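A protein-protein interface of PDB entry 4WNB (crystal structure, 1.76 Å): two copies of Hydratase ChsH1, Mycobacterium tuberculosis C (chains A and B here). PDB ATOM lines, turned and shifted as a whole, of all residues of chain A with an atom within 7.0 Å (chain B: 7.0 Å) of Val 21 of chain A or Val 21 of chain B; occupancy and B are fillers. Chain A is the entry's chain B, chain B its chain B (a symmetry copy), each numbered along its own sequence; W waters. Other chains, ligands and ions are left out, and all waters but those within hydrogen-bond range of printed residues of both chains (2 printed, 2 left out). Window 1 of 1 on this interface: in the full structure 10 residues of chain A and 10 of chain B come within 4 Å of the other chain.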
ATOM      1  N   ASP A  16      41.182 -17.278  -1.972  1.00  0.00           N
ATOM      2  CA  ASP A  16      40.656 -15.960  -2.283  1.00  0.00           C
ATOM      3  C   ASP A  16      39.128 -16.055  -2.350  1.00  0.00           C
ATOM      4  O   ASP A  16      38.573 -17.155  -2.465  1.00  0.00           O
ATOM      5  CB  ASP A  16      41.240 -15.446  -3.594  1.00  0.00           C
ATOM      6  CG  ASP A  16      41.141 -16.471  -4.692  1.00  0.00           C
ATOM      7  OD1 ASP A  16      40.077 -16.569  -5.325  1.00  0.00           O
ATOM      8  OD2 ASP A  16      42.116 -17.215  -4.889  1.00  0.00           O
ATOM      9  N   PRO A  17      38.440 -14.913  -2.219  1.00  0.00           N
ATOM     10  CA  PRO A  17      36.971 -14.949  -2.193  1.00  0.00           C
ATOM     11  C   PRO A  17      36.357 -15.642  -3.424  1.00  0.00           C
ATOM     12  O   PRO A  17      35.388 -16.390  -3.278  1.00  0.00           O
ATOM     13  CB  PRO A  17      36.601 -13.462  -2.116  1.00  0.00           C
ATOM     14  CG  PRO A  17      37.752 -12.885  -1.221  1.00  0.00           C
ATOM     15  CD  PRO A  17      38.969 -13.599  -1.790  1.00  0.00           C
ATOM     16  N   THR A  18      36.946 -15.448  -4.605  1.00  0.00           N
ATOM     17  CA  THR A  18      36.393 -16.055  -5.818  1.00  0.00           C
ATOM     18  C   THR A  18      36.434 -17.589  -5.680  1.00  0.00           C
ATOM     19  O   THR A  18      35.492 -18.295  -6.036  1.00  0.00           O
ATOM     20  CB  THR A  18      37.167 -15.605  -7.073  1.00  0.00           C
ATOM     21  OG1 THR A  18      37.013 -14.180  -7.246  1.00  0.00           O
ATOM     22  CG2 THR A  18      36.658 -16.347  -8.309  1.00  0.00           C
ATOM     23  N   PHE A  19      37.510 -18.101  -5.100  1.00  0.00           N
ATOM     24  CA  PHE A  19      37.601 -19.539  -4.918  1.00  0.00           C
ATOM     25  C   PHE A  19      36.525 -20.023  -3.942  1.00  0.00           C
ATOM     26  O   PHE A  19      35.831 -21.015  -4.194  1.00  0.00           O
ATOM     27  CB  PHE A  19      38.990 -19.936  -4.396  1.00  0.00           C
ATOM     28  CG  PHE A  19      39.097 -21.400  -4.037  1.00  0.00           C
ATOM     29  CD1 PHE A  19      39.386 -22.345  -4.998  1.00  0.00           C
ATOM     30  CD2 PHE A  19      38.902 -21.823  -2.731  1.00  0.00           C
ATOM     31  CE1 PHE A  19      39.475 -23.673  -4.682  1.00  0.00           C
ATOM     32  CE2 PHE A  19      38.992 -23.167  -2.424  1.00  0.00           C
ATOM     33  CZ  PHE A  19      39.271 -24.081  -3.391  1.00  0.00           C
ATOM     34  N   ILE A  20      36.422 -19.331  -2.810  1.00  0.00           N
ATOM     35  CA  ILE A  20      35.436 -19.716  -1.792  1.00  0.00           C
ATOM     36  C   ILE A  20      34.008 -19.658  -2.343  1.00  0.00           C
ATOM     37  O   ILE A  20      33.231 -20.600  -2.187  1.00  0.00           O
ATOM     38  CB  ILE A  20      35.570 -18.835  -0.546  1.00  0.00           C
ATOM     39  CG1 ILE A  20      36.924 -19.143   0.123  1.00  0.00           C
ATOM     40  CG2 ILE A  20      34.408 -19.109   0.443  1.00  0.00           C
ATOM     41  CD1 ILE A  20      37.194 -18.343   1.398  1.00  0.00           C
ATOM     42  N   VAL A  21      33.656 -18.557  -3.009  1.00  0.00           N
ATOM     43  CA  VAL A  21      32.308 -18.410  -3.562  1.00  0.00           C
ATOM     44  C   VAL A  21      32.010 -19.408  -4.718  1.00  0.00           C
ATOM     45  O   VAL A  21      30.940 -20.048  -4.773  1.00  0.00           O
ATOM     46  CB  VAL A  21      32.102 -16.977  -4.078  1.00  0.00           C
ATOM     47  CG1 VAL A  21      30.794 -16.854  -4.832  1.00  0.00           C
ATOM     48  CG2 VAL A  21      32.120 -15.981  -2.879  1.00  0.00           C
ATOM     49  N   SER A  22      32.935 -19.510  -5.666  1.00  0.00           N
ATOM     50  CA  SER A  22      32.679 -20.328  -6.853  1.00  0.00           C
ATOM     51  C   SER A  22      32.604 -21.813  -6.475  1.00  0.00           C
ATOM     52  O   SER A  22      31.786 -22.542  -7.020  1.00  0.00           O
ATOM     53  CB  SER A  22      33.741 -20.107  -7.920  1.00  0.00           C
ATOM     54  OG  SER A  22      35.032 -20.503  -7.492  1.00  0.00           O
ATOM     55  N   THR A  23      33.433 -22.244  -5.530  1.00  0.00           N
ATOM     56  CA  THR A  23      33.341 -23.651  -5.143  1.00  0.00           C
ATOM     57  C   THR A  23      32.028 -23.888  -4.380  1.00  0.00           C
ATOM     58  O   THR A  23      31.350 -24.889  -4.631  1.00  0.00           O
ATOM     59  CB  THR A  23      34.550 -24.114  -4.308  1.00  0.00           C
ATOM     60  OG1 THR A  23      34.722 -23.238  -3.180  1.00  0.00           O
ATOM     61  CG2 THR A  23      35.802 -24.103  -5.164  1.00  0.00           C
ATOM     62  N   ALA A  24      31.662 -22.998  -3.457  1.00  0.00           N
ATOM     63  CA  ALA A  24      30.421 -23.237  -2.714  1.00  0.00           C
ATOM     64  C   ALA A  24      29.228 -23.329  -3.680  1.00  0.00           C
ATOM     65  O   ALA A  24      28.405 -24.237  -3.570  1.00  0.00           O
ATOM     66  CB  ALA A  24      30.179 -22.142  -1.663  1.00  0.00           C
ATOM     67  N   LEU A  25      29.144 -22.409  -4.643  1.00  0.00           N
ATOM     68  CA  LEU A  25      27.964 -22.413  -5.506  1.00  0.00           C
ATOM     69  C   LEU A  25      28.035 -23.564  -6.513  1.00  0.00           C
ATOM     70  O   LEU A  25      26.987 -24.092  -6.912  1.00  0.00           O
ATOM     71  CB  LEU A  25      27.785 -21.055  -6.208  1.00  0.00           C
ATOM     72  CG  LEU A  25      26.815 -20.128  -5.443  1.00  0.00           C
ATOM     73  CD1 LEU A  25      27.402 -19.740  -4.088  1.00  0.00           C
ATOM     74  CD2 LEU A  25      26.478 -18.881  -6.257  1.00  0.00           C
ATOM     75  N   ALA A  26      29.245 -23.978  -6.901  1.00  0.00           N
ATOM     76  CA  ALA A  26      29.378 -25.177  -7.756  1.00  0.00           C
ATOM     77  C   ALA A  26      28.993 -26.482  -7.018  1.00  0.00           C
ATOM     78  O   ALA A  26      28.668 -27.486  -7.675  1.00  0.00           O
ATOM     79  CB  ALA A  26      30.797 -25.301  -8.310  1.00  0.00           C
ATOM     80  N   THR A  27      29.019 -26.465  -5.682  1.00  0.00           N
ATOM     81  CA  THR A  27      28.530 -27.622  -4.907  1.00  0.00           C
ATOM     82  C   THR A  27      27.060 -27.414  -4.496  1.00  0.00           C
ATOM     83  O   THR A  27      26.506 -28.205  -3.724  1.00  0.00           O
ATOM     84  CB  THR A  27      29.373 -27.899  -3.652  1.00  0.00           C
ATOM     85  OG1 THR A  27      29.296 -26.793  -2.738  1.00  0.00           O
ATOM     86  CG2 THR A  27      30.828 -28.159  -4.034  1.00  0.00           C
ATOM     87  N   ASP A  29      25.698 -25.143  -2.703  1.00  0.00           N
ATOM     88  CA  ASP A  29      25.593 -24.790  -1.304  1.00  0.00           C
ATOM     89  C   ASP A  29      25.422 -23.265  -1.236  1.00  0.00           C
ATOM     90  O   ASP A  29      26.382 -22.520  -1.471  1.00  0.00           O
ATOM     91  CB  ASP A  29      26.867 -25.227  -0.555  1.00  0.00           C
ATOM     92  CG  ASP A  29      26.809 -24.997   0.948  1.00  0.00           C
ATOM     93  OD1 ASP A  29      26.024 -24.166   1.450  1.00  0.00           O
ATOM     94  OD2 ASP A  29      27.626 -25.665   1.603  1.00  0.00           O
ATOM     95  N   PHE A  30      24.206 -22.815  -0.933  1.00  0.00           N
ATOM     96  CA  PHE A  30      23.901 -21.394  -0.990  1.00  0.00           C
ATOM     97  C   PHE A  30      23.864 -20.773   0.419  1.00  0.00           C
ATOM     98  O   PHE A  30      23.369 -19.639   0.587  1.00  0.00           O
ATOM     99  CB  PHE A  30      22.572 -21.191  -1.715  1.00  0.00           C
ATOM    100  CG  PHE A  30      22.641 -21.475  -3.203  1.00  0.00           C
ATOM    101  CD1 PHE A  30      23.012 -20.479  -4.104  1.00  0.00           C
ATOM    102  CD2 PHE A  30      22.377 -22.737  -3.680  1.00  0.00           C
ATOM    103  CE1 PHE A  30      23.089 -20.747  -5.479  1.00  0.00           C
ATOM    104  CE2 PHE A  30      22.450 -23.018  -5.049  1.00  0.00           C
ATOM    105  CZ  PHE A  30      22.809 -22.019  -5.945  1.00  0.00           C
ATOM    106  N   HIS A  34      29.265 -18.787   3.055  1.00  0.00           N
ATOM    107  CA  HIS A  34      30.301 -19.008   2.058  1.00  0.00           C
ATOM    108  C   HIS A  34      30.334 -17.924   0.988  1.00  0.00           C
ATOM    109  O   HIS A  34      31.190 -17.978   0.100  1.00  0.00           O
ATOM    110  CB  HIS A  34      30.141 -20.369   1.368  1.00  0.00           C
ATOM    111  CG  HIS A  34      29.783 -21.464   2.315  1.00  0.00           C
ATOM    112  ND1 HIS A  34      30.597 -21.832   3.363  1.00  0.00           N
ATOM    113  CD2 HIS A  34      28.698 -22.271   2.372  1.00  0.00           C
ATOM    114  CE1 HIS A  34      30.016 -22.805   4.048  1.00  0.00           C
ATOM    115  NE2 HIS A  34      28.855 -23.067   3.479  1.00  0.00           N
ATOM    116  N   HIS A  35      29.434 -16.940   1.058  1.00  0.00           N
ATOM    117  CA  HIS A  35      29.484 -15.847   0.076  1.00  0.00           C
ATOM    118  C   HIS A  35      29.085 -14.474   0.580  1.00  0.00           C
ATOM    119  O   HIS A  35      29.252 -13.499  -0.135  1.00  0.00           O
ATOM    120  CB  HIS A  35      28.613 -16.161  -1.145  1.00  0.00           C
ATOM    121  CG  HIS A  35      27.144 -16.230  -0.838  1.00  0.00           C
ATOM    122  ND1 HIS A  35      26.492 -17.419  -0.585  1.00  0.00           N
ATOM    123  CD2 HIS A  35      26.203 -15.257  -0.729  1.00  0.00           C
ATOM    124  CE1 HIS A  35      25.211 -17.181  -0.346  1.00  0.00           C
ATOM    125  NE2 HIS A  35      25.013 -15.876  -0.403  1.00  0.00           N
ATOM    126  N   ASP A  36      28.594 -14.384   1.805  1.00  0.00           N
ATOM    127  CA  ASP A  36      28.095 -13.119   2.331  1.00  0.00           C
ATOM    128  C   ASP A  36      28.869 -12.834   3.624  1.00  0.00           C
ATOM    129  O   ASP A  36      28.601 -13.394   4.684  1.00  0.00           O
ATOM    130  CB  ASP A  36      26.573 -13.206   2.547  1.00  0.00           C
ATOM    131  CG  ASP A  36      25.964 -11.919   3.107  1.00  0.00           C
ATOM    132  OD1 ASP A  36      26.705 -11.043   3.608  1.00  0.00           O
ATOM    133  OD2 ASP A  36      24.725 -11.795   3.037  1.00  0.00           O
ATOM    134  N   ILE A  48      33.865 -15.053   5.316  1.00  0.00           N
ATOM    135  CA  ILE A  48      33.339 -16.230   4.639  1.00  0.00           C
ATOM    136  C   ILE A  48      34.385 -17.348   4.699  1.00  0.00           C
ATOM    137  O   ILE A  48      35.595 -17.080   4.851  1.00  0.00           O
ATOM    138  CB  ILE A  48      32.981 -15.928   3.179  1.00  0.00           C
ATOM    139  CG1 ILE A  48      34.222 -15.436   2.428  1.00  0.00           C
ATOM    140  CG2 ILE A  48      31.843 -14.902   3.111  1.00  0.00           C
ATOM    141  CD1 ILE A  48      34.007 -15.375   0.909  1.00  0.00           C
ATOM    142  N   PHE A  49      33.939 -18.592   4.571  1.00  0.00           N
ATOM    143  CA  PHE A  49      34.851 -19.731   4.671  1.00  0.00           C
ATOM    144  C   PHE A  49      34.454 -20.869   3.741  1.00  0.00           C
ATOM    145  O   PHE A  49      33.294 -20.985   3.331  1.00  0.00           O
ATOM    146  CB  PHE A  49      34.948 -20.216   6.136  1.00  0.00           C
ATOM    147  CG  PHE A  49      33.616 -20.543   6.782  1.00  0.00           C
ATOM    148  CD1 PHE A  49      33.055 -21.814   6.651  1.00  0.00           C
ATOM    149  CD2 PHE A  49      32.947 -19.593   7.545  1.00  0.00           C
ATOM    150  CE1 PHE A  49      31.837 -22.131   7.265  1.00  0.00           C
ATOM    151  CE2 PHE A  49      31.726 -19.901   8.170  1.00  0.00           C
ATOM    152  CZ  PHE A  49      31.174 -21.183   8.022  1.00  0.00           C
ATOM    153  N   ASP B  16      20.100  -8.225  -1.803  1.00  0.00           N
ATOM    154  CA  ASP B  16      20.965  -8.769  -0.769  1.00  0.00           C
ATOM    155  C   ASP B  16      22.143  -9.475  -1.449  1.00  0.00           C
ATOM    156  O   ASP B  16      22.083  -9.783  -2.647  1.00  0.00           O
ATOM    157  CB  ASP B  16      20.188  -9.722   0.132  1.00  0.00           C
ATOM    158  CG  ASP B  16      19.400 -10.728  -0.664  1.00  0.00           C
ATOM    159  OD1 ASP B  16      19.975 -11.751  -1.076  1.00  0.00           O
ATOM    160  OD2 ASP B  16      18.212 -10.471  -0.922  1.00  0.00           O
ATOM    161  N   PRO B  17      23.239  -9.682  -0.708  1.00  0.00           N
ATOM    162  CA  PRO B  17      24.431 -10.280  -1.325  1.00  0.00           C
ATOM    163  C   PRO B  17      24.150 -11.634  -2.003  1.00  0.00           C
ATOM    164  O   PRO B  17      24.681 -11.892  -3.087  1.00  0.00           O
ATOM    165  CB  PRO B  17      25.394 -10.411  -0.137  1.00  0.00           C
ATOM    166  CG  PRO B  17      25.054  -9.129   0.699  1.00  0.00           C
ATOM    167  CD  PRO B  17      23.535  -9.107   0.624  1.00  0.00           C
ATOM    168  N   THR B  18      23.287 -12.459  -1.411  1.00  0.00           N
ATOM    169  CA  THR B  18      23.000 -13.774  -1.990  1.00  0.00           C
ATOM    170  C   THR B  18      22.371 -13.587  -3.383  1.00  0.00           C
ATOM    171  O   THR B  18      22.698 -14.288  -4.339  1.00  0.00           O
ATOM    172  CB  THR B  18      22.063 -14.595  -1.080  1.00  0.00           C
ATOM    173  OG1 THR B  18      22.725 -14.858   0.175  1.00  0.00           O
ATOM    174  CG2 THR B  18      21.675 -15.908  -1.760  1.00  0.00           C
ATOM    175  N   PHE B  19      21.506 -12.590  -3.512  1.00  0.00           N
ATOM    176  CA  PHE B  19      20.894 -12.345  -4.806  1.00  0.00           C
ATOM    177  C   PHE B  19      21.951 -11.903  -5.822  1.00  0.00           C
ATOM    178  O   PHE B  19      21.996 -12.397  -6.955  1.00  0.00           O
ATOM    179  CB  PHE B  19      19.800 -11.272  -4.697  1.00  0.00           C
ATOM    180  CG  PHE B  19      19.234 -10.858  -6.037  1.00  0.00           C
ATOM    181  CD1 PHE B  19      18.218 -11.578  -6.628  1.00  0.00           C
ATOM    182  CD2 PHE B  19      19.730  -9.747  -6.700  1.00  0.00           C
ATOM    183  CE1 PHE B  19      17.707 -11.216  -7.844  1.00  0.00           C
ATOM    184  CE2 PHE B  19      19.209  -9.392  -7.929  1.00  0.00           C
ATOM    185  CZ  PHE B  19      18.211 -10.122  -8.496  1.00  0.00           C
ATOM    186  N   ILE B  20      22.776 -10.943  -5.412  1.00  0.00           N
ATOM    187  CA  ILE B  20      23.819 -10.428  -6.310  1.00  0.00           C
ATOM    188  C   ILE B  20      24.789 -11.534  -6.736  1.00  0.00           C
ATOM    189  O   ILE B  20      25.084 -11.695  -7.920  1.00  0.00           O
ATOM    190  CB  ILE B  20      24.576  -9.269  -5.653  1.00  0.00           C
ATOM    191  CG1 ILE B  20      23.607  -8.081  -5.502  1.00  0.00           C
ATOM    192  CG2 ILE B  20      25.797  -8.859  -6.516  1.00  0.00           C
ATOM    193  CD1 ILE B  20      24.230  -6.836  -4.870  1.00  0.00           C
ATOM    194  N   VAL B  21      25.279 -12.319  -5.775  1.00  0.00           N
ATOM    195  CA  VAL B  21      26.221 -13.395  -6.089  1.00  0.00           C
ATOM    196  C   VAL B  21      25.584 -14.538  -6.929  1.00  0.00           C
ATOM    197  O   VAL B  21      26.163 -15.023  -7.923  1.00  0.00           O
ATOM    198  CB  VAL B  21      26.792 -13.991  -4.792  1.00  0.00           C
ATOM    199  CG1 VAL B  21      27.613 -15.232  -5.081  1.00  0.00           C
ATOM    200  CG2 VAL B  21      27.675 -12.928  -4.071  1.00  0.00           C
ATOM    201  N   SER B  22      24.412 -15.002  -6.509  1.00  0.00           N
ATOM    202  CA  SER B  22      23.805 -16.161  -7.165  1.00  0.00           C
ATOM    203  C   SER B  22      23.386 -15.806  -8.597  1.00  0.00           C
ATOM    204  O   SER B  22      23.527 -16.625  -9.495  1.00  0.00           O
ATOM    205  CB  SER B  22      22.611 -16.682  -6.378  1.00  0.00           C
ATOM    206  OG  SER B  22      21.561 -15.736  -6.294  1.00  0.00           O
ATOM    207  N   THR B  23      22.901 -14.587  -8.807  1.00  0.00           N
ATOM    208  CA  THR B  23      22.532 -14.235 -10.177  1.00  0.00           C
ATOM    209  C   THR B  23      23.803 -14.094 -11.031  1.00  0.00           C
ATOM    210  O   THR B  23      23.832 -14.579 -12.165  1.00  0.00           O
ATOM    211  CB  THR B  23      21.681 -12.953 -10.249  1.00  0.00           C
ATOM    212  OG1 THR B  23      22.358 -11.884  -9.564  1.00  0.00           O
ATOM    213  CG2 THR B  23      20.327 -13.197  -9.610  1.00  0.00           C
ATOM    214  N   ALA B  24      24.844 -13.439 -10.513  1.00  0.00           N
ATOM    215  CA  ALA B  24      26.047 -13.287 -11.336  1.00  0.00           C
ATOM    216  C   ALA B  24      26.599 -14.664 -11.740  1.00  0.00           C
ATOM    217  O   ALA B  24      26.927 -14.887 -12.904  1.00  0.00           O
ATOM    218  CB  ALA B  24      27.125 -12.470 -10.605  1.00  0.00           C
ATOM    219  N   LEU B  25      26.676 -15.598 -10.791  1.00  0.00           N
ATOM    220  CA  LEU B  25      27.295 -16.880 -11.126  1.00  0.00           C
ATOM    221  C   LEU B  25      26.351 -17.727 -11.983  1.00  0.00           C
ATOM    222  O   LEU B  25      26.822 -18.517 -12.813  1.00  0.00           O
ATOM    223  CB  LEU B  25      27.739 -17.631  -9.858  1.00  0.00           C
ATOM    224  CG  LEU B  25      29.225 -17.377  -9.522  1.00  0.00           C
ATOM    225  CD1 LEU B  25      29.446 -15.913  -9.150  1.00  0.00           C
ATOM    226  CD2 LEU B  25      29.706 -18.293  -8.399  1.00  0.00           C
ATOM    227  N   ALA B  26      25.035 -17.553 -11.819  1.00  0.00           N
ATOM    228  CA  ALA B  26      24.081 -18.236 -12.718  1.00  0.00           C
ATOM    229  C   ALA B  26      24.133 -17.693 -14.167  1.00  0.00           C
ATOM    230  O   ALA B  26      23.713 -18.396 -15.102  1.00  0.00           O
ATOM    231  CB  ALA B  26      22.653 -18.132 -12.183  1.00  0.00           C
ATOM    232  N   THR B  27      24.647 -16.473 -14.350  1.00  0.00           N
ATOM    233  CA  THR B  27      24.862 -15.945 -15.711  1.00  0.00           C
ATOM    234  C   THR B  27      26.310 -16.202 -16.168  1.00  0.00           C
ATOM    235  O   THR B  27      26.731 -15.716 -17.224  1.00  0.00           O
ATOM    236  CB  THR B  27      24.553 -14.443 -15.825  1.00  0.00           C
ATOM    237  OG1 THR B  27      25.446 -13.682 -14.996  1.00  0.00           O
ATOM    238  CG2 THR B  27      23.107 -14.164 -15.424  1.00  0.00           C
ATOM    239  N   ASP B  29      29.091 -15.224 -14.931  1.00  0.00           N
ATOM    240  CA  ASP B  29      29.880 -14.012 -14.871  1.00  0.00           C
ATOM    241  C   ASP B  29      30.693 -14.068 -13.569  1.00  0.00           C
ATOM    242  O   ASP B  29      30.133 -13.895 -12.478  1.00  0.00           O
ATOM    243  CB  ASP B  29      28.953 -12.781 -14.880  1.00  0.00           C
ATOM    244  CG  ASP B  29      29.692 -11.452 -14.928  1.00  0.00           C
ATOM    245  OD1 ASP B  29      30.883 -11.355 -14.565  1.00  0.00           O
ATOM    246  OD2 ASP B  29      29.002 -10.493 -15.312  1.00  0.00           O
ATOM    247  N   PHE B  30      31.994 -14.322 -13.689  1.00  0.00           N
ATOM    248  CA  PHE B  30      32.823 -14.545 -12.515  1.00  0.00           C
ATOM    249  C   PHE B  30      33.674 -13.304 -12.187  1.00  0.00           C
ATOM    250  O   PHE B  30      34.624 -13.394 -11.383  1.00  0.00           O
ATOM    251  CB  PHE B  30      33.705 -15.770 -12.743  1.00  0.00           C
ATOM    252  CG  PHE B  30      32.939 -17.080 -12.741  1.00  0.00           C
ATOM    253  CD1 PHE B  30      32.704 -17.767 -11.552  1.00  0.00           C
ATOM    254  CD2 PHE B  30      32.431 -17.587 -13.914  1.00  0.00           C
ATOM    255  CE1 PHE B  30      31.984 -18.971 -11.551  1.00  0.00           C
ATOM    256  CE2 PHE B  30      31.711 -18.787 -13.926  1.00  0.00           C
ATOM    257  CZ  PHE B  30      31.488 -19.475 -12.740  1.00  0.00           C
ATOM    258  N   HIS B  34      31.157  -8.685  -8.666  1.00  0.00           N
ATOM    259  CA  HIS B  34      29.825  -9.141  -8.300  1.00  0.00           C
ATOM    260  C   HIS B  34      29.835 -10.128  -7.139  1.00  0.00           C
ATOM    261  O   HIS B  34      28.764 -10.567  -6.711  1.00  0.00           O
ATOM    262  CB  HIS B  34      29.106  -9.794  -9.488  1.00  0.00           C
ATOM    263  CG  HIS B  34      29.308  -9.057 -10.768  1.00  0.00           C
ATOM    264  ND1 HIS B  34      28.902  -7.752 -10.943  1.00  0.00           N
ATOM    265  CD2 HIS B  34      29.872  -9.441 -11.936  1.00  0.00           C
ATOM    266  CE1 HIS B  34      29.235  -7.351 -12.160  1.00  0.00           C
ATOM    267  NE2 HIS B  34      29.844  -8.350 -12.767  1.00  0.00           N
ATOM    268  N   HIS B  35      31.013 -10.475  -6.615  1.00  0.00           N
ATOM    269  CA  HIS B  35      31.048 -11.374  -5.453  1.00  0.00           C
ATOM    270  C   HIS B  35      32.154 -11.129  -4.446  1.00  0.00           C
ATOM    271  O   HIS B  35      32.149 -11.733  -3.386  1.00  0.00           O
ATOM    272  CB  HIS B  35      31.141 -12.840  -5.891  1.00  0.00           C
ATOM    273  CG  HIS B  35      32.431 -13.183  -6.583  1.00  0.00           C
ATOM    274  ND1 HIS B  35      32.557 -13.197  -7.956  1.00  0.00           N
ATOM    275  CD2 HIS B  35      33.652 -13.512  -6.091  1.00  0.00           C
ATOM    276  CE1 HIS B  35      33.797 -13.529  -8.284  1.00  0.00           C
ATOM    277  NE2 HIS B  35      34.489 -13.703  -7.172  1.00  0.00           N
ATOM    278  N   ASP B  36      33.077 -10.231  -4.750  1.00  0.00           N
ATOM    279  CA  ASP B  36      34.227 -10.002  -3.884  1.00  0.00           C
ATOM    280  C   ASP B  36      34.230  -8.512  -3.522  1.00  0.00           C
ATOM    281  O   ASP B  36      34.629  -7.650  -4.300  1.00  0.00           O
ATOM    282  CB  ASP B  36      35.517 -10.449  -4.598  1.00  0.00           C
ATOM    283  CG  ASP B  36      36.779 -10.239  -3.762  1.00  0.00           C
ATOM    284  OD1 ASP B  36      36.745  -9.497  -2.754  1.00  0.00           O
ATOM    285  OD2 ASP B  36      37.814 -10.832  -4.129  1.00  0.00           O
ATOM    286  N   ILE B  48      29.887  -4.797  -3.819  1.00  0.00           N
ATOM    287  CA  ILE B  48      29.548  -5.598  -4.986  1.00  0.00           C
ATOM    288  C   ILE B  48      28.246  -5.068  -5.594  1.00  0.00           C
ATOM    289  O   ILE B  48      27.433  -4.425  -4.897  1.00  0.00           O
ATOM    290  CB  ILE B  48      29.391  -7.080  -4.627  1.00  0.00           C
ATOM    291  CG1 ILE B  48      28.292  -7.249  -3.574  1.00  0.00           C
ATOM    292  CG2 ILE B  48      30.726  -7.655  -4.138  1.00  0.00           C
ATOM    293  CD1 ILE B  48      27.892  -8.716  -3.367  1.00  0.00           C
ATOM    294  N   PHE B  49      28.032  -5.336  -6.877  1.00  0.00           N
ATOM    295  CA  PHE B  49      26.845  -4.826  -7.563  1.00  0.00           C
ATOM    296  C   PHE B  49      26.318  -5.803  -8.605  1.00  0.00           C
ATOM    297  O   PHE B  49      27.052  -6.662  -9.104  1.00  0.00           O
ATOM    298  CB  PHE B  49      27.139  -3.445  -8.192  1.00  0.00           C
ATOM    299  CG  PHE B  49      28.341  -3.416  -9.116  1.00  0.00           C
ATOM    300  CD1 PHE B  49      28.208  -3.734 -10.468  1.00  0.00           C
ATOM    301  CD2 PHE B  49      29.591  -3.036  -8.640  1.00  0.00           C
ATOM    302  CE1 PHE B  49      29.308  -3.686 -11.332  1.00  0.00           C
ATOM    303  CE2 PHE B  49      30.702  -2.978  -9.498  1.00  0.00           C
ATOM    304  CZ  PHE B  49      30.550  -3.310 -10.853  1.00  0.00           C
HETATM  305  O   HOH W   1      29.542 -11.252  -1.236  1.00  0.00           O
HETATM  306  O   HOH W   2      32.430 -12.672  -1.065  1.00  0.00           O
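A ring nitrogen (NE2) of His 35 of chain A sits at hydrogen-bond distance from the side-chain hydroxyl (OG1) of Thr 18 of chain B, at 2.6 Å.
A ring nitrogen (NE2) of His 35 of chain B lies within hydrogen-bond range of the side-chain hydroxyl (OG1) of Thr 18 of chain A (2.6 Å).
Water W1 lies within hydrogen-bond range of the backbone carbonyl oxygen (O) of His 35 of chain A (2.5 Å) and the backbone carbonyl oxygen (O) of His 35 of chain B (3.4 Å).
Water W2 bridges O of His 35 of chain B (2.5 Å) and O of His 35 of chain A (3.4 Å).
Among the printed residues, merely in contact across the chains: Pro 17 of chain A with Asp 36 of chain B (3.5 Å), Val 21 of chain A with Val 21 of chain B (3.6 Å), Val 21 of chain A with Leu 25 of chain B (3.997 Å), Ser 22 of chain A with Leu 25 of chain B (3.9 Å), Leu 25 of chain A with Val 21 of chain B (3.998 Å), Leu 25 of chain A with Ser 22 of chain B (3.9 Å), Leu 25 of chain A with Leu 25 of chain B (3.9 Å) and Asp 36 of chain A with Pro 17 of chain B (3.5 Å).
Of the 19 printed residues of chain B, 7 touch a printed residue of chain A.
Hydrophobic or aromatic side chains of chain B within 4 Å of the printed part of chain A: Pro 17, Val 21, Leu 25 and His 35.
Of the 19 printed residues of chain A, 7 touch a printed residue of chain B.
Hydrophobic or aromatic side chains of chain A that line the printed part of chain B: Pro 17, Val 21, Leu 25 and His 35.
Among the printed residues, 10 pairs touch across the chains.
Printed residues of chain B within 4 Å of Pro 17 of chain A: Asp 36 (3.5 Å).
Thr 23 of chain A touches none of the printed residues of chain B.
Of the printed residues of chain B, Leu 25 of chain A touches Val 21, Ser 22 and Leu 25.
Printed residues of chain B within 4 Å of Asp 36 of chain A: Pro 17 (3.5 Å).
Printed residues of chain A within 4 Å of Pro 17 of chain B: Asp 36.
N of Thr 18 of chain A lies close to OD1 of Asp 16 of chain A, at 3.4 Å.
O of Thr 18 of chain A is in hydrogen-bond range of OG of Ser 22 of chain A (2.7 Å).
N of Thr 18 of chain B sits close to OD1 of Asp 16 of chain B (3.4 Å).
O of Phe 19 of chain B is in hydrogen-bond range of OG of Ser 22 of chain B (3.4 Å).
OG of Ser 22 of chain A lies within hydrogen-bond range of O of Phe 19 of chain A (3.4 Å).
O of Thr 18 of chain B sits at hydrogen-bond distance from OG of Ser 22 of chain B (2.7 Å).
Thr 18 of chain A touches His 35 of chain B, and with the chains exchanged His 35 of chain A touches Thr 18 of chain B.
Val 21 of chain A touches Leu 25 of chain B, and with the chains exchanged Leu 25 of chain A touches Val 21 of chain B.
Ser 22 of chain A touches Leu 25 of chain B, and with the chains exchanged Leu 25 of chain A touches Ser 22 of chain B.
Leu 25 of chain A touches its own counterpart, Leu 25 of chain B.
Positions printed for both chains: 16, 17, 18, 19, 20, 21, 22, 23, 24, 25, 26, 27, 29, 30, 34, 35, 36, 48 and 49.
Of the 10 pairs that touch across the chains among the printed residues, 10 have their exchanged pair printed and touching as well.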
